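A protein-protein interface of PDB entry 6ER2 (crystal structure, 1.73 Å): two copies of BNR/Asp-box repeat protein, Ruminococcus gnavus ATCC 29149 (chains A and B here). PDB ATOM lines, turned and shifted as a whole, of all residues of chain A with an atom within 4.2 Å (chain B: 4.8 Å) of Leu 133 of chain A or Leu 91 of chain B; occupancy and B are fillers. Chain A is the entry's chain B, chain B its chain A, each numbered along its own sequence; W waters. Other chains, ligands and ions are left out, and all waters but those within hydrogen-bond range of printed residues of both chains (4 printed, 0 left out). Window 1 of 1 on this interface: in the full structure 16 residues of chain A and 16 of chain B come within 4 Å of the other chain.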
ATOM      1  N   THR A  90      -8.585 -15.480 -21.252  1.00  0.00           N
ATOM      2  CA  THR A  90      -7.440 -15.139 -20.435  1.00  0.00           C
ATOM      3  C   THR A  90      -7.365 -13.624 -20.243  1.00  0.00           C
ATOM      4  O   THR A  90      -7.797 -12.835 -21.088  1.00  0.00           O
ATOM      5  CB  THR A  90      -6.153 -15.615 -21.111  1.00  0.00           C
ATOM      6  OG1 THR A  90      -6.024 -14.892 -22.331  1.00  0.00           O
ATOM      7  CG2 THR A  90      -6.127 -17.129 -21.398  1.00  0.00           C
ATOM      8  N   LEU A  91      -6.802 -13.236 -19.110  1.00  0.00           N
ATOM      9  CA  LEU A  91      -6.321 -11.877 -18.933  1.00  0.00           C
ATOM     10  C   LEU A  91      -5.001 -12.020 -18.251  1.00  0.00           C
ATOM     11  O   LEU A  91      -4.885 -12.783 -17.314  1.00  0.00           O
ATOM     12  CB  LEU A  91      -7.203 -10.996 -18.055  1.00  0.00           C
ATOM     13  CG  LEU A  91      -8.545 -10.502 -18.609  1.00  0.00           C
ATOM     14  CD1 LEU A  91      -9.493  -9.920 -17.559  1.00  0.00           C
ATOM     15  CD2 LEU A  91      -8.205  -9.452 -19.666  1.00  0.00           C
ATOM     16  N   LYS A 119     -21.450  -9.486 -20.565  1.00  0.00           N
ATOM     17  CA  LYS A 119     -20.494 -10.390 -21.210  1.00  0.00           C
ATOM     18  C   LYS A 119     -19.073  -9.925 -21.049  1.00  0.00           C
ATOM     19  O   LYS A 119     -18.310  -9.909 -22.025  1.00  0.00           O
ATOM     20  CB  LYS A 119     -20.853 -10.618 -22.677  1.00  0.00           C
ATOM     21  CG  LYS A 119     -22.263 -11.143 -22.861  1.00  0.00           C
ATOM     22  CD  LYS A 119     -22.402 -11.836 -24.184  1.00  0.00           C
ATOM     23  CE  LYS A 119     -22.764 -10.892 -25.283  1.00  0.00           C
ATOM     24  NZ  LYS A 119     -22.897 -11.651 -26.555  1.00  0.00           N
ATOM     25  N   GLN A 120     -18.766  -9.470 -19.837  1.00  0.00           N
ATOM     26  CA  GLN A 120     -17.510  -8.798 -19.505  1.00  0.00           C
ATOM     27  C   GLN A 120     -16.820  -9.420 -18.298  1.00  0.00           C
ATOM     28  O   GLN A 120     -17.472  -9.831 -17.347  1.00  0.00           O
ATOM     29  CB  GLN A 120     -17.772  -7.331 -19.154  1.00  0.00           C
ATOM     30  CG  GLN A 120     -17.697  -6.389 -20.285  1.00  0.00           C
ATOM     31  CD  GLN A 120     -17.917  -4.951 -19.859  1.00  0.00           C
ATOM     32  OE1 GLN A 120     -18.535  -4.644 -18.814  1.00  0.00           O
ATOM     33  NE2 GLN A 120     -17.411  -4.061 -20.676  1.00  0.00           N
ATOM     34  N   TYR A 121     -15.491  -9.420 -18.343  1.00  0.00           N
ATOM     35  CA  TYR A 121     -14.607  -9.776 -17.250  1.00  0.00           C
ATOM     36  C   TYR A 121     -13.737  -8.554 -17.005  1.00  0.00           C
ATOM     37  O   TYR A 121     -13.195  -8.001 -17.966  1.00  0.00           O
ATOM     38  CB  TYR A 121     -13.686 -10.947 -17.594  1.00  0.00           C
ATOM     39  CG  TYR A 121     -14.422 -12.112 -18.228  1.00  0.00           C
ATOM     40  CD1 TYR A 121     -14.620 -12.144 -19.593  1.00  0.00           C
ATOM     41  CD2 TYR A 121     -14.888 -13.180 -17.467  1.00  0.00           C
ATOM     42  CE1 TYR A 121     -15.269 -13.220 -20.191  1.00  0.00           C
ATOM     43  CE2 TYR A 121     -15.566 -14.232 -18.051  1.00  0.00           C
ATOM     44  CZ  TYR A 121     -15.744 -14.249 -19.413  1.00  0.00           C
ATOM     45  OH  TYR A 121     -16.401 -15.303 -20.008  1.00  0.00           O
ATOM     46  N   THR A 132     -10.049  -5.176 -19.123  1.00  0.00           N
ATOM     47  CA  THR A 132     -11.434  -5.598 -19.357  1.00  0.00           C
ATOM     48  C   THR A 132     -11.449  -6.493 -20.596  1.00  0.00           C
ATOM     49  O   THR A 132     -10.840  -6.160 -21.588  1.00  0.00           O
ATOM     50  CB  THR A 132     -12.352  -4.392 -19.612  1.00  0.00           C
ATOM     51  OG1 THR A 132     -12.262  -3.470 -18.505  1.00  0.00           O
ATOM     52  CG2 THR A 132     -13.821  -4.822 -19.862  1.00  0.00           C
ATOM     53  N   LEU A 133     -12.187  -7.595 -20.517  1.00  0.00           N
ATOM     54  CA  LEU A 133     -12.395  -8.484 -21.638  1.00  0.00           C
ATOM     55  C   LEU A 133     -13.891  -8.613 -21.932  1.00  0.00           C
ATOM     56  O   LEU A 133     -14.655  -8.940 -21.023  1.00  0.00           O
ATOM     57  CB  LEU A 133     -11.779  -9.858 -21.317  1.00  0.00           C
ATOM     58  CG  LEU A 133     -12.041 -11.000 -22.332  1.00  0.00           C
ATOM     59  CD1 LEU A 133     -11.407 -10.677 -23.680  1.00  0.00           C
ATOM     60  CD2 LEU A 133     -11.507 -12.305 -21.779  1.00  0.00           C
ATOM     61  N   ASP A 134     -14.284  -8.405 -23.188  1.00  0.00           N
ATOM     62  CA  ASP A 134     -15.644  -8.733 -23.640  1.00  0.00           C
ATOM     63  C   ASP A 134     -15.570  -9.835 -24.680  1.00  0.00           C
ATOM     64  O   ASP A 134     -14.815  -9.727 -25.634  1.00  0.00           O
ATOM     65  CB  ASP A 134     -16.413  -7.521 -24.178  1.00  0.00           C
ATOM     66  CG  ASP A 134     -17.894  -7.855 -24.476  1.00  0.00           C
ATOM     67  OD1 ASP A 134     -18.171  -8.714 -25.355  1.00  0.00           O
ATOM     68  OD2 ASP A 134     -18.799  -7.266 -23.826  1.00  0.00           O
ATOM     69  N   GLN A 135     -16.285 -10.916 -24.442  1.00  0.00           N
ATOM     70  CA  GLN A 135     -16.356 -12.041 -25.379  1.00  0.00           C
ATOM     71  C   GLN A 135     -17.780 -12.199 -25.854  1.00  0.00           C
ATOM     72  O   GLN A 135     -18.689 -12.230 -25.030  1.00  0.00           O
ATOM     73  CB  GLN A 135     -15.945 -13.334 -24.697  1.00  0.00           C
ATOM     74  CG  GLN A 135     -14.463 -13.501 -24.473  1.00  0.00           C
ATOM     75  CD  GLN A 135     -13.598 -13.818 -25.686  1.00  0.00           C
ATOM     76  OE1 GLN A 135     -12.389 -13.666 -25.569  1.00  0.00           O
ATOM     77  NE2 GLN A 135     -14.168 -14.283 -26.812  1.00  0.00           N
ATOM     78  N   TYR B  69      -3.965 -15.486 -35.463  1.00  0.00           N
ATOM     79  CA  TYR B  69      -4.053 -16.893 -35.783  1.00  0.00           C
ATOM     80  C   TYR B  69      -5.475 -17.428 -35.850  1.00  0.00           C
ATOM     81  O   TYR B  69      -6.457 -16.820 -35.385  1.00  0.00           O
ATOM     82  CB  TYR B  69      -3.224 -17.682 -34.765  1.00  0.00           C
ATOM     83  CG  TYR B  69      -3.797 -17.643 -33.357  1.00  0.00           C
ATOM     84  CD1 TYR B  69      -4.790 -18.549 -32.955  1.00  0.00           C
ATOM     85  CD2 TYR B  69      -3.328 -16.748 -32.423  1.00  0.00           C
ATOM     86  CE1 TYR B  69      -5.323 -18.521 -31.680  1.00  0.00           C
ATOM     87  CE2 TYR B  69      -3.856 -16.727 -31.131  1.00  0.00           C
ATOM     88  CZ  TYR B  69      -4.857 -17.606 -30.773  1.00  0.00           C
ATOM     89  OH  TYR B  69      -5.357 -17.590 -29.485  1.00  0.00           O
ATOM     90  N   VAL B  76     -10.500 -18.075 -33.656  1.00  0.00           N
ATOM     91  CA  VAL B  76      -9.676 -16.968 -34.132  1.00  0.00           C
ATOM     92  C   VAL B  76      -9.052 -16.309 -32.909  1.00  0.00           C
ATOM     93  O   VAL B  76      -9.690 -16.210 -31.879  1.00  0.00           O
ATOM     94  CB  VAL B  76     -10.530 -15.924 -34.897  1.00  0.00           C
ATOM     95  CG1 VAL B  76      -9.619 -14.841 -35.471  1.00  0.00           C
ATOM     96  CG2 VAL B  76     -11.374 -16.564 -36.009  1.00  0.00           C
ATOM     97  N   GLY B  77      -7.800 -15.869 -33.011  1.00  0.00           N
ATOM     98  CA  GLY B  77      -7.192 -15.197 -31.885  1.00  0.00           C
ATOM     99  C   GLY B  77      -5.966 -14.415 -32.240  1.00  0.00           C
ATOM    100  O   GLY B  77      -5.549 -14.401 -33.383  1.00  0.00           O
ATOM    101  N   MET B  78      -5.406 -13.756 -31.239  1.00  0.00           N
ATOM    102  CA  MET B  78      -4.098 -13.135 -31.387  1.00  0.00           C
ATOM    103  C   MET B  78      -3.301 -13.280 -30.113  1.00  0.00           C
ATOM    104  O   MET B  78      -3.879 -13.446 -29.049  1.00  0.00           O
ATOM    105  CB  MET B  78      -4.250 -11.682 -31.764  1.00  0.00           C
ATOM    106  CG  MET B  78      -4.739 -10.771 -30.673  1.00  0.00           C
ATOM    107  SD  MET B  78      -3.312 -10.022 -29.835  1.00  0.00           S
ATOM    108  CE  MET B  78      -4.135  -9.140 -28.514  1.00  0.00           C
ATOM    109  N   TYR B  89      -0.261 -10.771 -24.009  1.00  0.00           N
ATOM    110  CA  TYR B  89      -1.641 -10.387 -24.262  1.00  0.00           C
ATOM    111  C   TYR B  89      -2.191 -11.365 -25.274  1.00  0.00           C
ATOM    112  O   TYR B  89      -1.663 -11.463 -26.366  1.00  0.00           O
ATOM    113  CB  TYR B  89      -1.749  -8.952 -24.764  1.00  0.00           C
ATOM    114  CG  TYR B  89      -1.339  -7.867 -23.772  1.00  0.00           C
ATOM    115  CD1 TYR B  89      -1.178  -8.138 -22.406  1.00  0.00           C
ATOM    116  CD2 TYR B  89      -1.149  -6.555 -24.198  1.00  0.00           C
ATOM    117  CE1 TYR B  89      -0.834  -7.141 -21.522  1.00  0.00           C
ATOM    118  CE2 TYR B  89      -0.796  -5.552 -23.309  1.00  0.00           C
ATOM    119  CZ  TYR B  89      -0.621  -5.854 -21.981  1.00  0.00           C
ATOM    120  OH  TYR B  89      -0.297  -4.851 -21.095  1.00  0.00           O
ATOM    121  N   THR B  90      -3.288 -12.024 -24.914  1.00  0.00           N
ATOM    122  CA  THR B  90      -3.870 -13.131 -25.715  1.00  0.00           C
ATOM    123  C   THR B  90      -5.346 -12.831 -25.858  1.00  0.00           C
ATOM    124  O   THR B  90      -6.002 -12.548 -24.852  1.00  0.00           O
ATOM    125  CB  THR B  90      -3.744 -14.511 -24.995  1.00  0.00           C
ATOM    126  OG1 THR B  90      -2.379 -14.835 -24.694  1.00  0.00           O
ATOM    127  CG2 THR B  90      -4.339 -15.688 -25.837  1.00  0.00           C
ATOM    128  N   LEU B  91      -5.903 -12.944 -27.065  1.00  0.00           N
ATOM    129  CA  LEU B  91      -7.341 -12.855 -27.236  1.00  0.00           C
ATOM    130  C   LEU B  91      -7.692 -14.083 -28.059  1.00  0.00           C
ATOM    131  O   LEU B  91      -7.200 -14.231 -29.145  1.00  0.00           O
ATOM    132  CB  LEU B  91      -7.666 -11.530 -27.922  1.00  0.00           C
ATOM    133  CG  LEU B  91      -9.026 -10.950 -27.929  1.00  0.00           C
ATOM    134  CD1 LEU B  91      -9.705 -10.979 -26.571  1.00  0.00           C
ATOM    135  CD2 LEU B  91      -9.068  -9.547 -28.541  1.00  0.00           C
ATOM    136  N   ASP B  92      -8.473 -14.996 -27.517  1.00  0.00           N
ATOM    137  CA  ASP B  92      -8.783 -16.261 -28.196  1.00  0.00           C
ATOM    138  C   ASP B  92     -10.275 -16.472 -28.191  1.00  0.00           C
ATOM    139  O   ASP B  92     -10.883 -16.475 -27.135  1.00  0.00           O
ATOM    140  CB  ASP B  92      -8.081 -17.434 -27.509  1.00  0.00           C
ATOM    141  CG  ASP B  92      -8.212 -18.733 -28.306  1.00  0.00           C
ATOM    142  OD1 ASP B  92      -9.189 -19.479 -28.099  1.00  0.00           O
ATOM    143  OD2 ASP B  92      -7.372 -18.973 -29.179  1.00  0.00           O
ATOM    144  N   CYS B  93     -10.872 -16.608 -29.380  1.00  0.00           N
ATOM    145  CA  CYS B  93     -12.325 -16.677 -29.533  1.00  0.00           C
ATOM    146  C   CYS B  93     -12.707 -18.004 -30.163  1.00  0.00           C
ATOM    147  O   CYS B  93     -12.255 -18.319 -31.276  1.00  0.00           O
ATOM    148  CB  CYS B  93     -12.818 -15.570 -30.438  1.00  0.00           C
ATOM    149  SG  CYS B  93     -12.426 -13.946 -29.805  1.00  0.00           S
ATOM    150  N   TYR B 121      -7.986  -3.593 -28.076  1.00  0.00           N
ATOM    151  CA  TYR B 121      -7.832  -4.552 -29.191  1.00  0.00           C
ATOM    152  C   TYR B 121      -9.185  -5.129 -29.472  1.00  0.00           C
ATOM    153  O   TYR B 121      -9.895  -5.497 -28.526  1.00  0.00           O
ATOM    154  CB  TYR B 121      -6.890  -5.705 -28.821  1.00  0.00           C
ATOM    155  CG  TYR B 121      -5.591  -5.277 -28.171  1.00  0.00           C
ATOM    156  CD1 TYR B 121      -4.463  -4.971 -28.937  1.00  0.00           C
ATOM    157  CD2 TYR B 121      -5.487  -5.161 -26.785  1.00  0.00           C
ATOM    158  CE1 TYR B 121      -3.259  -4.596 -28.336  1.00  0.00           C
ATOM    159  CE2 TYR B 121      -4.295  -4.775 -26.189  1.00  0.00           C
ATOM    160  CZ  TYR B 121      -3.191  -4.465 -26.972  1.00  0.00           C
ATOM    161  OH  TYR B 121      -2.013  -4.080 -26.358  1.00  0.00           O
ATOM    162  N   LEU B 123     -11.268  -7.875 -32.136  1.00  0.00           N
ATOM    163  CA  LEU B 123     -11.228  -8.925 -33.140  1.00  0.00           C
ATOM    164  C   LEU B 123     -12.577  -9.082 -33.828  1.00  0.00           C
ATOM    165  O   LEU B 123     -13.617  -9.091 -33.159  1.00  0.00           O
ATOM    166  CB  LEU B 123     -10.847 -10.201 -32.424  1.00  0.00           C
ATOM    167  CG  LEU B 123     -10.307 -11.372 -33.192  1.00  0.00           C
ATOM    168  CD1 LEU B 123      -8.961 -11.083 -33.879  1.00  0.00           C
ATOM    169  CD2 LEU B 123     -10.128 -12.499 -32.184  1.00  0.00           C
ATOM    170  N   ALA B 131     -14.698 -10.073 -30.015  1.00  0.00           N
ATOM    171  CA  ALA B 131     -14.118  -9.816 -28.715  1.00  0.00           C
ATOM    172  C   ALA B 131     -13.449  -8.483 -28.649  1.00  0.00           C
ATOM    173  O   ALA B 131     -12.955  -7.985 -29.663  1.00  0.00           O
ATOM    174  CB  ALA B 131     -13.108 -10.899 -28.336  1.00  0.00           C
ATOM    175  N   THR B 132     -13.389  -7.930 -27.434  1.00  0.00           N
ATOM    176  CA  THR B 132     -12.701  -6.676 -27.192  1.00  0.00           C
ATOM    177  C   THR B 132     -11.849  -6.852 -25.930  1.00  0.00           C
ATOM    178  O   THR B 132     -12.325  -7.385 -24.949  1.00  0.00           O
ATOM    179  CB  THR B 132     -13.686  -5.510 -26.959  1.00  0.00           C
ATOM    180  OG1 THR B 132     -14.571  -5.397 -28.092  1.00  0.00           O
ATOM    181  CG2 THR B 132     -12.937  -4.170 -26.708  1.00  0.00           C
ATOM    182  N   LEU B 133     -10.606  -6.410 -25.999  1.00  0.00           N
ATOM    183  CA  LEU B 133      -9.685  -6.429 -24.863  1.00  0.00           C
ATOM    184  C   LEU B 133      -9.243  -4.982 -24.582  1.00  0.00           C
ATOM    185  O   LEU B 133      -8.716  -4.302 -25.472  1.00  0.00           O
ATOM    186  CB  LEU B 133      -8.490  -7.330 -25.170  1.00  0.00           C
ATOM    187  CG  LEU B 133      -7.352  -7.332 -24.146  1.00  0.00           C
ATOM    188  CD1 LEU B 133      -7.815  -7.849 -22.798  1.00  0.00           C
ATOM    189  CD2 LEU B 133      -6.163  -8.143 -24.672  1.00  0.00           C
HETATM  190  O   HOH W   1     -13.277  -5.043 -23.203  1.00  0.00           O
HETATM  191  O   HOH W   2      -7.989 -11.604 -23.392  1.00  0.00           O
HETATM  192  O   HOH W   3      -7.649 -15.397 -24.551  1.00  0.00           O
HETATM  193  O   HOH W   4     -16.619  -7.352 -27.982  1.00  0.00           O
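The backbone carbonyl oxygen (O) of Thr 90 of chain B is in hydrogen-bond range of the side-chain hydroxyl (OG1) of Thr 90 of chain A.
SG of Cys 93 of chain B sits at hydrogen-bond distance from NE2 of Gln 135 of chain A, 3.5 Å away.
N of Asp 134 of chain A sits at hydrogen-bond distance from O of Thr 132 of chain B (2.8 Å).
The side-chain carboxylate (OD2) of Asp 92 of chain B is in hydrogen-bond range of the side-chain hydroxyl (OH) of Tyr 69 of chain B.
The backbone NH of Cys 93 of chain B lies within hydrogen-bond range of the backbone carbonyl oxygen of Val 76 of chain B, at 2.8 Å.
N of Met 78 of chain B is in hydrogen-bond range of O of Leu 91 of chain B (2.8 Å).
The backbone carbonyl oxygen of Tyr 121 of chain B is in hydrogen-bond range of the backbone NH of Leu 133 of chain B (2.8 Å).
N of Leu 123 of chain B lies within hydrogen-bond range of O of Ala 131 of chain B.
The backbone NH (N) of Leu 133 of chain A sits at hydrogen-bond distance from the backbone carbonyl oxygen (O) of Tyr 121 of chain A (2.8 Å).
Among the printed residues, merely in contact across the chains: Asp 134 of chain A with Ala 131 of chain B, Leu 133 of chain A with Leu 91 of chain B, Thr 132 of chain A with Leu 133 of chain B, Leu 133 of chain A with Thr 132 of chain B, Leu 91 of chain A with Leu 133 of chain B, Gln 135 of chain A with Asp 92 of chain B, Gln 135 of chain A with Ala 131 of chain B, Thr 132 of chain A with Thr 132 of chain B and Gln 135 of chain A with Leu 91 of chain B.
Leu 133 of chain A touches just these residues of chain B: Leu 91 (3.4 Å) and Thr 132 (3.5 Å).
Of chain A, only Leu 133 (3.4 Å) and Gln 135 (3.9 Å) come within 4 Å of Leu 91 of chain B.
Of the printed residues of chain A, Asp 92 of chain B touches Gln 135.
Of the printed residues of chain A, Cys 93 of chain B touches Gln 135.
Printed residues of chain A within 4 Å of Thr 132 of chain B: Thr 132, Leu 133 and Asp 134.
The nearest printed residue of chain A that does not touch Leu 91 of chain B is Thr 90 of chain A (5.1 Å).
The nearest printed residue of chain B that does not touch Asp 134 of chain A is Leu 133 of chain B (5.0 Å).
Printed residues of chain A that touch a printed residue of chain B: Thr 90, Leu 91, Thr 132, Leu 133, Asp 134 and Gln 135.
Hydrophobic or aromatic side chains of chain A within 4 Å of the printed part of chain B: Leu 91 and Leu 133.
Printed residues of chain B that touch a printed residue of chain A: Thr 90, Leu 91, Asp 92, Cys 93, Ala 131, Thr 132 and Leu 133.
Among the printed residues, 12 pairs touch across the chains.
Among the printed residues, no Asp or Glu carboxylate lies within 4 Å of a Lys or Arg side-chain nitrogen of the other chain.
Thr 90 of chain B touches its own counterpart, Thr 90 of chain A.
Leu 91 of chain A touches Leu 133 of chain B, and with the chains exchanged Leu 133 of chain A touches Leu 91 of chain B.
Thr 132 of chain B touches its own counterpart, Thr 132 of chain A.
Thr 132 of chain A touches Leu 133 of chain B, and with the chains exchanged Leu 133 of chain A touches Thr 132 of chain B.
5 positions are printed for both chains.
Of the 12 pairs that touch across the chains among the printed residues, 6 have their exchanged pair printed and touching as well.
Water W2 bridges O of Thr 90 of chain A (2.6 Å) and O of Thr 90 of chain B (2.6 Å).
Water W3 lies within hydrogen-bond range of the side-chain hydroxyl (OG1) of Thr 90 of chain A, the backbone NH (N) of Asp 92 of chain B and the backbone carbonyl oxygen (O) of Thr 90 of chain B.
Water W4 lies within hydrogen-bond range of OG1 of Thr 132 of chain B (2.8 Å) and OD1 of Asp 134 of chain A (3.3 Å).
Water W1 lies within hydrogen-bond range of O of Thr 132 of chain B (3.1 Å) and O of Thr 132 of chain A (3.1 Å).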
